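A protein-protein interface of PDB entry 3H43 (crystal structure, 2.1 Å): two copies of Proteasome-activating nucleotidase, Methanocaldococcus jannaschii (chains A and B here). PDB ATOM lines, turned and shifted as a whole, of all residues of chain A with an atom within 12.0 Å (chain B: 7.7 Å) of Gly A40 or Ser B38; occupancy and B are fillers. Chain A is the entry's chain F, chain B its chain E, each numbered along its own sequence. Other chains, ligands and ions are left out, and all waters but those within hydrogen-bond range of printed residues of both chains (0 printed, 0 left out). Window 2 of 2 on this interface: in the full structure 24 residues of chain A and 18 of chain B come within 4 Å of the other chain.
Gly A40 touches Ser B38, but with the chains exchanged Ser A38 does not touch Gly B40 (11.5 Å). Pro A41 touches Ser B38, but with the chains exchanged Ser A38 does not touch Pro B41 (13.8 Å). Phe A43 touches Leu B19, but with the chains exchanged Leu A19 does not touch Phe B43 (23.2 Å). Phe A43 touches Val B21, but with the chains exchanged Val A21 does not touch Phe B43 (19.7 Å).
Hydrophobic or aromatic side chains of chain A that line the printed part of chain B: Val A34, Pro A41, Phe A43 and Leu A44. Of the 15 printed residues of chain B, 5 touch a printed residue of chain A. Printed residues of chain B that touch a printed residue of chain A: Leu B19, Ile B20, Val B21, Ser B38 and Thr B39. Among the printed residues, no Asp or Glu carboxylate lies within 4 Å of a Lys or Arg side-chain nitrogen of the other chain.
The backbone carbonyl oxygen of Ile B20 is in hydrogen-bond range of the backbone NH of Leu B64 (2.6 Å). O of Val B21 is in hydrogen-bond range of OG of Ser B38 (2.7 Å). OG of Ser B37 sits at hydrogen-bond distance from OG1 of Thr B39 (2.5 Å). The backbone carbonyl oxygen (O) of Val A34 sits at hydrogen-bond distance from the backbone NH (N) of Val A25 (2.8 Å). The backbone NH of Val A34 is in hydrogen-bond range of the backbone carbonyl oxygen of Asp A26, at 2.8 Å. The backbone carbonyl oxygen of Phe A43 sits at hydrogen-bond distance from the backbone NH of Val A35.
The backbone NH of Leu A44 lies within hydrogen-bond range of the backbone carbonyl oxygen of Leu B19 (2.7 Å). The backbone NH (N) of Val B21 sits at hydrogen-bond distance from the backbone carbonyl oxygen (O) of Ser A42. The backbone NH (N) of Ser A42 lies within hydrogen-bond range of the side-chain hydroxyl (OG) of Ser B38, at 2.7 Å.
Gly A40 touches one residue of chain B. Ser B38 touches just these residues of chain A: Gly A40 (3.7 Å), Pro A41 (3.3 Å) and Ser A42 (2.7 Å). Of chain B, only Ser B38 (3.3 Å) and Thr B39 (3.2 Å) come within 4 Å of Pro A41. Of chain A, only Ser A42 (3.6 Å) and Phe A43 (3.6 Å) come within 4 Å of Ile B20. Of chain A, only Val A34 (3.8 Å), Ser A42 (2.9 Å), Phe A43 (3.95 Å) and Leu A44 (3.9 Å) come within 4 Å of Val B21. No residue of chain A comes within 4 Å of Gly B22. No residue of chain A comes within 4 Å of Ser B37. Of the printed residues of chain A, Thr B39 touches Pro A41. No residue of chain A comes within 4 Å of Gly B40. Printed residues of chain B within 4 Å of Ser A42: Ile B20 (3.6 Å), Val B21 (2.9 Å) and Ser B38 (2.7 Å). Of the printed residues of chain B, Phe A43 touches Leu B19 (3.1 Å), Ile B20 (3.6 Å) and Val B21 (3.95 Å). Printed residues of chain B within 4 Å of Val A34: Val B21. Pro B41 touches none of the printed residues of chain A. The nearest residue of chain B that does not touch Gly A40 is Thr B39 (5.1 Å). The nearest printed residue of chain B that does not touch Ser A42 is Leu B19 (4.2 Å).
CG1 of Val A34 touches CG2 of Val B21 (3.8 Å). Gly A40 touches Ser B38 (O to O, 3.7 Å). CA of Pro A41 touches O of Ser B38, at 3.3 Å. CG2 of Thr B39 touches CB of Pro A41, at 3.2 Å. O of Ser A42 touches CA of Ile B20, at 3.6 Å. O of Leu B19 touches CA of Phe A43 (3.1 Å). CE2 of Phe A43 touches CG1 of Ile B20 (3.6 Å). Phe A43 touches Val B21. N of Leu A44 touches CG2 of Val B21 (3.9 Å).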
ATOM      1  N   LEU A  19     -27.799  11.794 -19.660  1.00  0.00           N
ATOM      2  CA  LEU A  19     -27.303  10.817 -20.607  1.00  0.00           C
ATOM      3  C   LEU A  19     -26.451   9.844 -19.800  1.00  0.00           C
ATOM      4  O   LEU A  19     -25.866  10.214 -18.778  1.00  0.00           O
ATOM      5  CB  LEU A  19     -26.479  11.505 -21.691  1.00  0.00           C
ATOM      6  CG  LEU A  19     -27.268  12.524 -22.531  1.00  0.00           C
ATOM      7  CD1 LEU A  19     -26.348  13.266 -23.485  1.00  0.00           C
ATOM      8  CD2 LEU A  19     -28.348  11.818 -23.288  1.00  0.00           C
ATOM      9  N   ILE A  20     -26.410   8.589 -20.232  1.00  0.00           N
ATOM     10  CA  ILE A  20     -25.625   7.601 -19.521  1.00  0.00           C
ATOM     11  C   ILE A  20     -24.217   7.626 -20.100  1.00  0.00           C
ATOM     12  O   ILE A  20     -24.040   7.825 -21.297  1.00  0.00           O
ATOM     13  CB  ILE A  20     -26.230   6.194 -19.679  1.00  0.00           C
ATOM     14  CG1 ILE A  20     -27.590   6.145 -18.988  1.00  0.00           C
ATOM     15  CG2 ILE A  20     -25.303   5.147 -19.065  1.00  0.00           C
ATOM     16  CD1 ILE A  20     -28.426   4.949 -19.379  1.00  0.00           C
ATOM     17  N   VAL A  21     -23.217   7.482 -19.243  1.00  0.00           N
ATOM     18  CA  VAL A  21     -21.848   7.471 -19.721  1.00  0.00           C
ATOM     19  C   VAL A  21     -21.429   6.020 -19.929  1.00  0.00           C
ATOM     20  O   VAL A  21     -21.723   5.152 -19.113  1.00  0.00           O
ATOM     21  CB  VAL A  21     -20.874   8.138 -18.731  1.00  0.00           C
ATOM     22  CG1 VAL A  21     -19.446   8.023 -19.266  1.00  0.00           C
ATOM     23  CG2 VAL A  21     -21.248   9.618 -18.538  1.00  0.00           C
ATOM     24  N   GLY A  22     -20.772   5.760 -21.049  1.00  0.00           N
ATOM     25  CA  GLY A  22     -20.298   4.420 -21.334  1.00  0.00           C
ATOM     26  C   GLY A  22     -18.912   4.481 -21.955  1.00  0.00           C
ATOM     27  O   GLY A  22     -18.383   5.571 -22.216  1.00  0.00           O
ATOM     28  N   THR A  23     -18.313   3.311 -22.160  1.00  0.00           N
ATOM     29  CA  THR A  23     -16.981   3.216 -22.759  1.00  0.00           C
ATOM     30  C   THR A  23     -17.047   2.304 -23.984  1.00  0.00           C
ATOM     31  O   THR A  23     -17.602   1.205 -23.916  1.00  0.00           O
ATOM     32  CB  THR A  23     -15.937   2.615 -21.770  1.00  0.00           C
ATOM     33  OG1 THR A  23     -15.991   3.314 -20.520  1.00  0.00           O
ATOM     34  CG2 THR A  23     -14.527   2.745 -22.347  1.00  0.00           C
ATOM     35  N   VAL A  24     -16.500   2.772 -25.097  1.00  0.00           N
ATOM     36  CA  VAL A  24     -16.483   1.988 -26.326  1.00  0.00           C
ATOM     37  C   VAL A  24     -15.608   0.760 -26.098  1.00  0.00           C
ATOM     38  O   VAL A  24     -14.476   0.873 -25.632  1.00  0.00           O
ATOM     39  CB  VAL A  24     -15.889   2.799 -27.515  1.00  0.00           C
ATOM     40  CG1 VAL A  24     -15.653   1.874 -28.724  1.00  0.00           C
ATOM     41  CG2 VAL A  24     -16.833   3.915 -27.912  1.00  0.00           C
ATOM     42  N   VAL A  25     -16.142  -0.418 -26.392  1.00  0.00           N
ATOM     43  CA  VAL A  25     -15.359  -1.636 -26.247  1.00  0.00           C
ATOM     44  C   VAL A  25     -14.698  -1.874 -27.594  1.00  0.00           C
ATOM     45  O   VAL A  25     -13.496  -2.104 -27.673  1.00  0.00           O
ATOM     46  CB  VAL A  25     -16.233  -2.842 -25.887  1.00  0.00           C
ATOM     47  CG1 VAL A  25     -15.385  -4.113 -25.892  1.00  0.00           C
ATOM     48  CG2 VAL A  25     -16.876  -2.625 -24.512  1.00  0.00           C
ATOM     49  N   ASP A  26     -15.500  -1.791 -28.652  1.00  0.00           N
ATOM     50  CA  ASP A  26     -15.014  -1.970 -30.007  1.00  0.00           C
ATOM     51  C   ASP A  26     -16.071  -1.532 -31.005  1.00  0.00           C
ATOM     52  O   ASP A  26     -17.267  -1.578 -30.718  1.00  0.00           O
ATOM     53  CB  ASP A  26     -14.646  -3.436 -30.266  1.00  0.00           C
ATOM     54  CG  ASP A  26     -15.814  -4.383 -30.042  1.00  0.00           C
ATOM     55  OD1 ASP A  26     -16.285  -4.486 -28.890  1.00  0.00           O
ATOM     56  OD2 ASP A  26     -16.263  -5.026 -31.015  1.00  0.00           O
ATOM     57  N   VAL A  33     -21.334   0.182 -32.460  1.00  0.00           N
ATOM     58  CA  VAL A  33     -20.251  -0.084 -31.520  1.00  0.00           C
ATOM     59  C   VAL A  33     -20.796  -0.882 -30.354  1.00  0.00           C
ATOM     60  O   VAL A  33     -21.994  -0.832 -30.056  1.00  0.00           O
ATOM     61  CB  VAL A  33     -19.642   1.215 -30.917  1.00  0.00           C
ATOM     62  CG1 VAL A  33     -18.976   2.040 -31.988  1.00  0.00           C
ATOM     63  CG2 VAL A  33     -20.712   2.018 -30.214  1.00  0.00           C
ATOM     64  N   VAL A  34     -19.924  -1.643 -29.710  1.00  0.00           N
ATOM     65  CA  VAL A  34     -20.328  -2.357 -28.517  1.00  0.00           C
ATOM     66  C   VAL A  34     -19.826  -1.375 -27.462  1.00  0.00           C
ATOM     67  O   VAL A  34     -18.666  -0.955 -27.501  1.00  0.00           O
ATOM     68  CB  VAL A  34     -19.594  -3.694 -28.354  1.00  0.00           C
ATOM     69  CG1 VAL A  34     -19.875  -4.286 -26.966  1.00  0.00           C
ATOM     70  CG2 VAL A  34     -20.047  -4.666 -29.425  1.00  0.00           C
ATOM     71  N   VAL A  35     -20.701  -0.958 -26.559  1.00  0.00           N
ATOM     72  CA  VAL A  35     -20.287  -0.037 -25.512  1.00  0.00           C
ATOM     73  C   VAL A  35     -20.533  -0.680 -24.154  1.00  0.00           C
ATOM     74  O   VAL A  35     -21.514  -1.402 -23.955  1.00  0.00           O
ATOM     75  CB  VAL A  35     -21.061   1.301 -25.562  1.00  0.00           C
ATOM     76  CG1 VAL A  35     -20.703   2.072 -26.829  1.00  0.00           C
ATOM     77  CG2 VAL A  35     -22.558   1.036 -25.488  1.00  0.00           C
ATOM     78  N   LYS A  36     -19.619  -0.452 -23.223  1.00  0.00           N
ATOM     79  CA  LYS A  36     -19.824  -0.996 -21.897  1.00  0.00           C
ATOM     80  C   LYS A  36     -20.420   0.161 -21.127  1.00  0.00           C
ATOM     81  O   LYS A  36     -19.759   1.167 -20.906  1.00  0.00           O
ATOM     82  CB  LYS A  36     -18.518  -1.440 -21.248  1.00  0.00           C
ATOM     83  CG  LYS A  36     -18.752  -2.039 -19.869  1.00  0.00           C
ATOM     84  CD  LYS A  36     -17.460  -2.440 -19.185  1.00  0.00           C
ATOM     85  CE  LYS A  36     -17.737  -2.985 -17.784  1.00  0.00           C
ATOM     86  NZ  LYS A  36     -18.444  -1.982 -16.924  1.00  0.00           N
ATOM     87  N   SER A  37     -21.684   0.019 -20.756  1.00  0.00           N
ATOM     88  CA  SER A  37     -22.388   1.057 -20.016  1.00  0.00           C
ATOM     89  C   SER A  37     -21.840   1.165 -18.605  1.00  0.00           C
ATOM     90  O   SER A  37     -21.411   0.170 -18.022  1.00  0.00           O
ATOM     91  CB  SER A  37     -23.885   0.735 -19.941  1.00  0.00           C
ATOM     92  OG  SER A  37     -24.554   1.663 -19.103  1.00  0.00           O
ATOM     93  N   SER A  38     -21.851   2.372 -18.051  1.00  0.00           N
ATOM     94  CA  SER A  38     -21.380   2.520 -16.686  1.00  0.00           C
ATOM     95  C   SER A  38     -22.437   1.879 -15.761  1.00  0.00           C
ATOM     96  O   SER A  38     -22.221   1.754 -14.558  1.00  0.00           O
ATOM     97  CB  SER A  38     -21.155   4.008 -16.339  1.00  0.00           C
ATOM     98  OG  SER A  38     -22.342   4.772 -16.467  1.00  0.00           O
ATOM     99  N   THR A  39     -23.573   1.475 -16.337  1.00  0.00           N
ATOM    100  CA  THR A  39     -24.638   0.827 -15.568  1.00  0.00           C
ATOM    101  C   THR A  39     -24.390  -0.679 -15.436  1.00  0.00           C
ATOM    102  O   THR A  39     -25.162  -1.380 -14.768  1.00  0.00           O
ATOM    103  CB  THR A  39     -26.044   1.002 -16.204  1.00  0.00           C
ATOM    104  OG1 THR A  39     -26.071   0.383 -17.500  1.00  0.00           O
ATOM    105  CG2 THR A  39     -26.412   2.480 -16.315  1.00  0.00           C
ATOM    106  N   GLY A  40     -23.334  -1.177 -16.080  1.00  0.00           N
ATOM    107  CA  GLY A  40     -23.022  -2.597 -15.976  1.00  0.00           C
ATOM    108  C   GLY A  40     -22.860  -3.391 -17.269  1.00  0.00           C
ATOM    109  O   GLY A  40     -21.747  -3.690 -17.677  1.00  0.00           O
ATOM    110  N   PRO A  41     -23.959  -3.750 -17.933  1.00  0.00           N
ATOM    111  CA  PRO A  41     -23.922  -4.521 -19.180  1.00  0.00           C
ATOM    112  C   PRO A  41     -23.311  -3.834 -20.396  1.00  0.00           C
ATOM    113  O   PRO A  41     -23.116  -2.616 -20.423  1.00  0.00           O
ATOM    114  CB  PRO A  41     -25.387  -4.869 -19.411  1.00  0.00           C
ATOM    115  CG  PRO A  41     -26.110  -3.704 -18.808  1.00  0.00           C
ATOM    116  CD  PRO A  41     -25.344  -3.452 -17.531  1.00  0.00           C
ATOM    117  N   SER A  42     -22.970  -4.646 -21.388  1.00  0.00           N
ATOM    118  CA  SER A  42     -22.424  -4.126 -22.637  1.00  0.00           C
ATOM    119  C   SER A  42     -23.532  -4.276 -23.674  1.00  0.00           C
ATOM    120  O   SER A  42     -24.296  -5.249 -23.651  1.00  0.00           O
ATOM    121  CB  SER A  42     -21.184  -4.904 -23.058  1.00  0.00           C
ATOM    122  OG  SER A  42     -20.066  -4.475 -22.311  1.00  0.00           O
ATOM    123  N   PHE A  43     -23.622  -3.300 -24.567  1.00  0.00           N
ATOM    124  CA  PHE A  43     -24.648  -3.278 -25.601  1.00  0.00           C
ATOM    125  C   PHE A  43     -24.104  -3.018 -27.010  1.00  0.00           C
ATOM    126  O   PHE A  43     -23.066  -2.376 -27.180  1.00  0.00           O
ATOM    127  CB  PHE A  43     -25.663  -2.170 -25.304  1.00  0.00           C
ATOM    128  CG  PHE A  43     -26.435  -2.361 -24.033  1.00  0.00           C
ATOM    129  CD1 PHE A  43     -25.924  -1.918 -22.810  1.00  0.00           C
ATOM    130  CD2 PHE A  43     -27.690  -2.962 -24.063  1.00  0.00           C
ATOM    131  CE1 PHE A  43     -26.668  -2.071 -21.631  1.00  0.00           C
ATOM    132  CE2 PHE A  43     -28.446  -3.125 -22.892  1.00  0.00           C
ATOM    133  CZ  PHE A  43     -27.937  -2.680 -21.676  1.00  0.00           C
ATOM    134  N   LEU A  44     -24.811  -3.528 -28.015  1.00  0.00           N
ATOM    135  CA  LEU A  44     -24.456  -3.260 -29.411  1.00  0.00           C
ATOM    136  C   LEU A  44     -25.431  -2.117 -29.719  1.00  0.00           C
ATOM    137  O   LEU A  44     -26.654  -2.307 -29.717  1.00  0.00           O
ATOM    138  CB  LEU A  44     -24.755  -4.456 -30.321  1.00  0.00           C
ATOM    139  CG  LEU A  44     -24.492  -4.160 -31.810  1.00  0.00           C
ATOM    140  CD1 LEU A  44     -23.027  -3.854 -32.004  1.00  0.00           C
ATOM    141  CD2 LEU A  44     -24.880  -5.349 -32.692  1.00  0.00           C
ATOM    142  N   VAL A  45     -24.891  -0.932 -29.952  1.00  0.00           N
ATOM    143  CA  VAL A  45     -25.719   0.239 -30.192  1.00  0.00           C
ATOM    144  C   VAL A  45     -25.320   0.992 -31.456  1.00  0.00           C
ATOM    145  O   VAL A  45     -24.235   0.793 -31.998  1.00  0.00           O
ATOM    146  CB  VAL A  45     -25.637   1.215 -28.982  1.00  0.00           C
ATOM    147  CG1 VAL A  45     -25.951   0.465 -27.684  1.00  0.00           C
ATOM    148  CG2 VAL A  45     -24.241   1.836 -28.900  1.00  0.00           C
ATOM    149  N   ARG A  61     -14.854   7.426 -23.893  1.00  0.00           N
ATOM    150  CA  ARG A  61     -16.066   7.567 -23.101  1.00  0.00           C
ATOM    151  C   ARG A  61     -17.091   8.258 -23.993  1.00  0.00           C
ATOM    152  O   ARG A  61     -16.773   9.221 -24.689  1.00  0.00           O
ATOM    153  CB  ARG A  61     -15.772   8.396 -21.855  1.00  0.00           C
ATOM    154  CG  ARG A  61     -14.705   7.764 -20.983  1.00  0.00           C
ATOM    155  CD  ARG A  61     -13.958   8.808 -20.173  1.00  0.00           C
ATOM    156  NE  ARG A  61     -14.800   9.492 -19.194  1.00  0.00           N
ATOM    157  CZ  ARG A  61     -15.467   8.880 -18.219  1.00  0.00           C
ATOM    158  NH1 ARG A  61     -15.400   7.561 -18.091  1.00  0.00           N
ATOM    159  NH2 ARG A  61     -16.183   9.589 -17.356  1.00  0.00           N
ATOM    160  N   VAL A  62     -18.316   7.754 -23.973  1.00  0.00           N
ATOM    161  CA  VAL A  62     -19.386   8.289 -24.809  1.00  0.00           C
ATOM    162  C   VAL A  62     -20.667   8.533 -24.013  1.00  0.00           C
ATOM    163  O   VAL A  62     -20.831   8.011 -22.910  1.00  0.00           O
ATOM    164  CB  VAL A  62     -19.702   7.297 -25.962  1.00  0.00           C
ATOM    165  CG1 VAL A  62     -18.537   7.261 -26.957  1.00  0.00           C
ATOM    166  CG2 VAL A  62     -19.936   5.892 -25.379  1.00  0.00           C
ATOM    167  N   LEU A  64     -24.720   8.100 -23.869  1.00  0.00           N
ATOM    168  CA  LEU A  64     -25.768   7.260 -24.420  1.00  0.00           C
ATOM    169  C   LEU A  64     -27.174   7.740 -24.075  1.00  0.00           C
ATOM    170  O   LEU A  64     -27.467   8.044 -22.914  1.00  0.00           O
ATOM    171  CB  LEU A  64     -25.600   5.829 -23.884  1.00  0.00           C
ATOM    172  CG  LEU A  64     -24.200   5.204 -23.943  1.00  0.00           C
ATOM    173  CD1 LEU A  64     -24.240   3.785 -23.351  1.00  0.00           C
ATOM    174  CD2 LEU A  64     -23.709   5.177 -25.381  1.00  0.00           C
ATOM    175  N   LEU A  69     -29.845   3.911 -25.770  1.00  0.00           N
ATOM    176  CA  LEU A  69     -28.408   3.755 -25.596  1.00  0.00           C
ATOM    177  C   LEU A  69     -27.649   4.142 -26.846  1.00  0.00           C
ATOM    178  O   LEU A  69     -26.455   3.850 -26.972  1.00  0.00           O
ATOM    179  CB  LEU A  69     -28.043   2.324 -25.216  1.00  0.00           C
ATOM    180  CG  LEU A  69     -28.529   1.917 -23.827  1.00  0.00           C
ATOM    181  CD1 LEU A  69     -28.183   0.470 -23.553  1.00  0.00           C
ATOM    182  CD2 LEU A  69     -27.887   2.824 -22.796  1.00  0.00           C
ATOM    183  N   LEU B  19     -29.016  -4.149 -28.434  1.00  0.00           N
ATOM    184  CA  LEU B  19     -28.877  -5.567 -28.148  1.00  0.00           C
ATOM    185  C   LEU B  19     -27.847  -5.724 -27.028  1.00  0.00           C
ATOM    186  O   LEU B  19     -26.860  -4.985 -26.964  1.00  0.00           O
ATOM    187  CB  LEU B  19     -28.405  -6.325 -29.395  1.00  0.00           C
ATOM    188  CG  LEU B  19     -29.244  -6.243 -30.688  1.00  0.00           C
ATOM    189  CD1 LEU B  19     -28.457  -6.902 -31.812  1.00  0.00           C
ATOM    190  CD2 LEU B  19     -30.600  -6.946 -30.513  1.00  0.00           C
ATOM    191  N   ILE B  20     -28.091  -6.678 -26.140  1.00  0.00           N
ATOM    192  CA  ILE B  20     -27.173  -6.967 -25.051  1.00  0.00           C
ATOM    193  C   ILE B  20     -26.069  -7.900 -25.576  1.00  0.00           C
ATOM    194  O   ILE B  20     -26.341  -8.853 -26.303  1.00  0.00           O
ATOM    195  CB  ILE B  20     -27.908  -7.664 -23.891  1.00  0.00           C
ATOM    196  CG1 ILE B  20     -28.957  -6.707 -23.314  1.00  0.00           C
ATOM    197  CG2 ILE B  20     -26.906  -8.135 -22.815  1.00  0.00           C
ATOM    198  CD1 ILE B  20     -29.889  -7.359 -22.341  1.00  0.00           C
ATOM    199  N   VAL B  21     -24.828  -7.612 -25.221  1.00  0.00           N
ATOM    200  CA  VAL B  21     -23.719  -8.440 -25.653  1.00  0.00           C
ATOM    201  C   VAL B  21     -23.366  -9.380 -24.532  1.00  0.00           C
ATOM    202  O   VAL B  21     -23.331  -8.982 -23.385  1.00  0.00           O
ATOM    203  CB  VAL B  21     -22.492  -7.592 -26.003  1.00  0.00           C
ATOM    204  CG1 VAL B  21     -21.287  -8.491 -26.259  1.00  0.00           C
ATOM    205  CG2 VAL B  21     -22.803  -6.745 -27.226  1.00  0.00           C
ATOM    206  N   GLY B  22     -23.149 -10.640 -24.870  1.00  0.00           N
ATOM    207  CA  GLY B  22     -22.783 -11.612 -23.863  1.00  0.00           C
ATOM    208  C   GLY B  22     -21.749 -12.548 -24.452  1.00  0.00           C
ATOM    209  O   GLY B  22     -21.323 -12.373 -25.592  1.00  0.00           O
ATOM    210  N   THR B  23     -21.352 -13.548 -23.681  1.00  0.00           N
ATOM    211  CA  THR B  23     -20.375 -14.511 -24.135  1.00  0.00           C
ATOM    212  C   THR B  23     -20.936 -15.917 -23.981  1.00  0.00           C
ATOM    213  O   THR B  23     -21.537 -16.250 -22.959  1.00  0.00           O
ATOM    214  CB  THR B  23     -19.085 -14.388 -23.322  1.00  0.00           C
ATOM    215  OG1 THR B  23     -18.609 -13.046 -23.416  1.00  0.00           O
ATOM    216  CG2 THR B  23     -18.015 -15.327 -23.862  1.00  0.00           C
ATOM    217  N   VAL B  35     -25.292 -18.423 -21.870  1.00  0.00           N
ATOM    218  CA  VAL B  35     -24.488 -17.258 -22.183  1.00  0.00           C
ATOM    219  C   VAL B  35     -24.273 -16.488 -20.894  1.00  0.00           C
ATOM    220  O   VAL B  35     -25.169 -16.437 -20.037  1.00  0.00           O
ATOM    221  CB  VAL B  35     -25.215 -16.349 -23.202  1.00  0.00           C
ATOM    222  CG1 VAL B  35     -25.427 -17.104 -24.528  1.00  0.00           C
ATOM    223  CG2 VAL B  35     -26.569 -15.934 -22.647  1.00  0.00           C
ATOM    224  N   LYS B  36     -23.083 -15.923 -20.735  1.00  0.00           N
ATOM    225  CA  LYS B  36     -22.814 -15.130 -19.555  1.00  0.00           C
ATOM    226  C   LYS B  36     -23.034 -13.719 -20.030  1.00  0.00           C
ATOM    227  O   LYS B  36     -22.261 -13.173 -20.817  1.00  0.00           O
ATOM    228  CB  LYS B  36     -21.386 -15.289 -19.053  1.00  0.00           C
ATOM    229  CG  LYS B  36     -21.170 -14.530 -17.760  1.00  0.00           C
ATOM    230  CD  LYS B  36     -19.769 -14.703 -17.217  1.00  0.00           C
ATOM    231  CE  LYS B  36     -19.579 -13.883 -15.953  1.00  0.00           C
ATOM    232  NZ  LYS B  36     -18.169 -13.930 -15.489  1.00  0.00           N
ATOM    233  N   SER B  37     -24.129 -13.144 -19.565  1.00  0.00           N
ATOM    234  CA  SER B  37     -24.492 -11.801 -19.943  1.00  0.00           C
ATOM    235  C   SER B  37     -23.567 -10.796 -19.292  1.00  0.00           C
ATOM    236  O   SER B  37     -23.014 -11.028 -18.217  1.00  0.00           O
ATOM    237  CB  SER B  37     -25.940 -11.524 -19.529  1.00  0.00           C
ATOM    238  OG  SER B  37     -26.315 -10.199 -19.842  1.00  0.00           O
ATOM    239  N   SER B  38     -23.386  -9.678 -19.976  1.00  0.00           N
ATOM    240  CA  SER B  38     -22.565  -8.605 -19.459  1.00  0.00           C
ATOM    241  C   SER B  38     -23.396  -7.955 -18.339  1.00  0.00           C
ATOM    242  O   SER B  38     -22.870  -7.198 -17.519  1.00  0.00           O
ATOM    243  CB  SER B  38     -22.275  -7.611 -20.576  1.00  0.00           C
ATOM    244  OG  SER B  38     -23.480  -7.297 -21.238  1.00  0.00           O
ATOM    245  N   THR B  39     -24.696  -8.261 -18.310  1.00  0.00           N
ATOM    246  CA  THR B  39     -25.565  -7.724 -17.265  1.00  0.00           C
ATOM    247  C   THR B  39     -25.205  -8.362 -15.917  1.00  0.00           C
ATOM    248  O   THR B  39     -25.647  -7.888 -14.869  1.00  0.00           O
ATOM    249  CB  THR B  39     -27.090  -7.967 -17.550  1.00  0.00           C
ATOM    250  OG1 THR B  39     -27.353  -9.370 -17.695  1.00  0.00           O
ATOM    251  CG2 THR B  39     -27.530  -7.231 -18.804  1.00  0.00           C
ATOM    252  N   GLY B  40     -24.405  -9.433 -15.954  1.00  0.00           N
ATOM    253  CA  GLY B  40     -23.984 -10.099 -14.727  1.00  0.00           C
ATOM    254  C   GLY B  40     -24.155 -11.609 -14.648  1.00  0.00           C
ATOM    255  O   GLY B  40     -23.186 -12.367 -14.700  1.00  0.00           O
ATOM    256  N   PRO B  41     -25.392 -12.082 -14.520  1.00  0.00           N
ATOM    257  CA  PRO B  41     -25.655 -13.516 -14.424  1.00  0.00           C
ATOM    258  C   PRO B  41     -25.525 -14.309 -15.724  1.00  0.00           C
ATOM    259  O   PRO B  41     -25.290 -13.750 -16.798  1.00  0.00           O
ATOM    260  CB  PRO B  41     -27.075 -13.558 -13.865  1.00  0.00           C
ATOM    261  CG  PRO B  41     -27.706 -12.343 -14.475  1.00  0.00           C
ATOM    262  CD  PRO B  41     -26.630 -11.296 -14.361  1.00  0.00           C
ATOM    263  N   PHE B  43     -27.410 -17.133 -18.263  1.00  0.00           N
ATOM    264  CA  PHE B  43     -28.757 -17.566 -18.631  1.00  0.00           C
ATOM    265  C   PHE B  43     -28.749 -18.666 -19.685  1.00  0.00           C
ATOM    266  O   PHE B  43     -27.825 -18.765 -20.491  1.00  0.00           O
ATOM    267  CB  PHE B  43     -29.589 -16.432 -19.253  1.00  0.00           C
ATOM    268  CG  PHE B  43     -29.748 -15.220 -18.395  1.00  0.00           C
ATOM    269  CD1 PHE B  43     -28.706 -14.305 -18.251  1.00  0.00           C
ATOM    270  CD2 PHE B  43     -30.968 -14.951 -17.775  1.00  0.00           C
ATOM    271  CE1 PHE B  43     -28.876 -13.136 -17.507  1.00  0.00           C
ATOM    272  CE2 PHE B  43     -31.146 -13.778 -17.024  1.00  0.00           C
ATOM    273  CZ  PHE B  43     -30.101 -12.876 -16.892  1.00  0.00           C
ATOM    274  N   VAL B  62     -21.942 -12.915 -28.366  1.00  0.00           N
ATOM    275  CA  VAL B  62     -23.225 -12.920 -29.050  1.00  0.00           C
ATOM    276  C   VAL B  62     -24.065 -11.696 -28.701  1.00  0.00           C
ATOM    277  O   VAL B  62     -23.798 -11.006 -27.715  1.00  0.00           O
ATOM    278  CB  VAL B  62     -24.034 -14.189 -28.696  1.00  0.00           C
ATOM    279  CG1 VAL B  62     -23.425 -15.406 -29.380  1.00  0.00           C
ATOM    280  CG2 VAL B  62     -24.066 -14.387 -27.191  1.00  0.00           C
ATOM    281  N   LEU B  64     -27.844 -10.432 -27.783  1.00  0.00           N
ATOM    282  CA  LEU B  64     -29.070 -10.967 -27.222  1.00  0.00           C
ATOM    283  C   LEU B  64     -30.214  -9.968 -27.306  1.00  0.00           C
ATOM    284  O   LEU B  64     -30.015  -8.774 -27.055  1.00  0.00           O
ATOM    285  CB  LEU B  64     -28.816 -11.341 -25.744  1.00  0.00           C
ATOM    286  CG  LEU B  64     -27.543 -12.160 -25.530  1.00  0.00           C
ATOM    287  CD1 LEU B  64     -27.224 -12.297 -24.056  1.00  0.00           C
ATOM    288  CD2 LEU B  64     -27.720 -13.526 -26.189  1.00  0.00           C
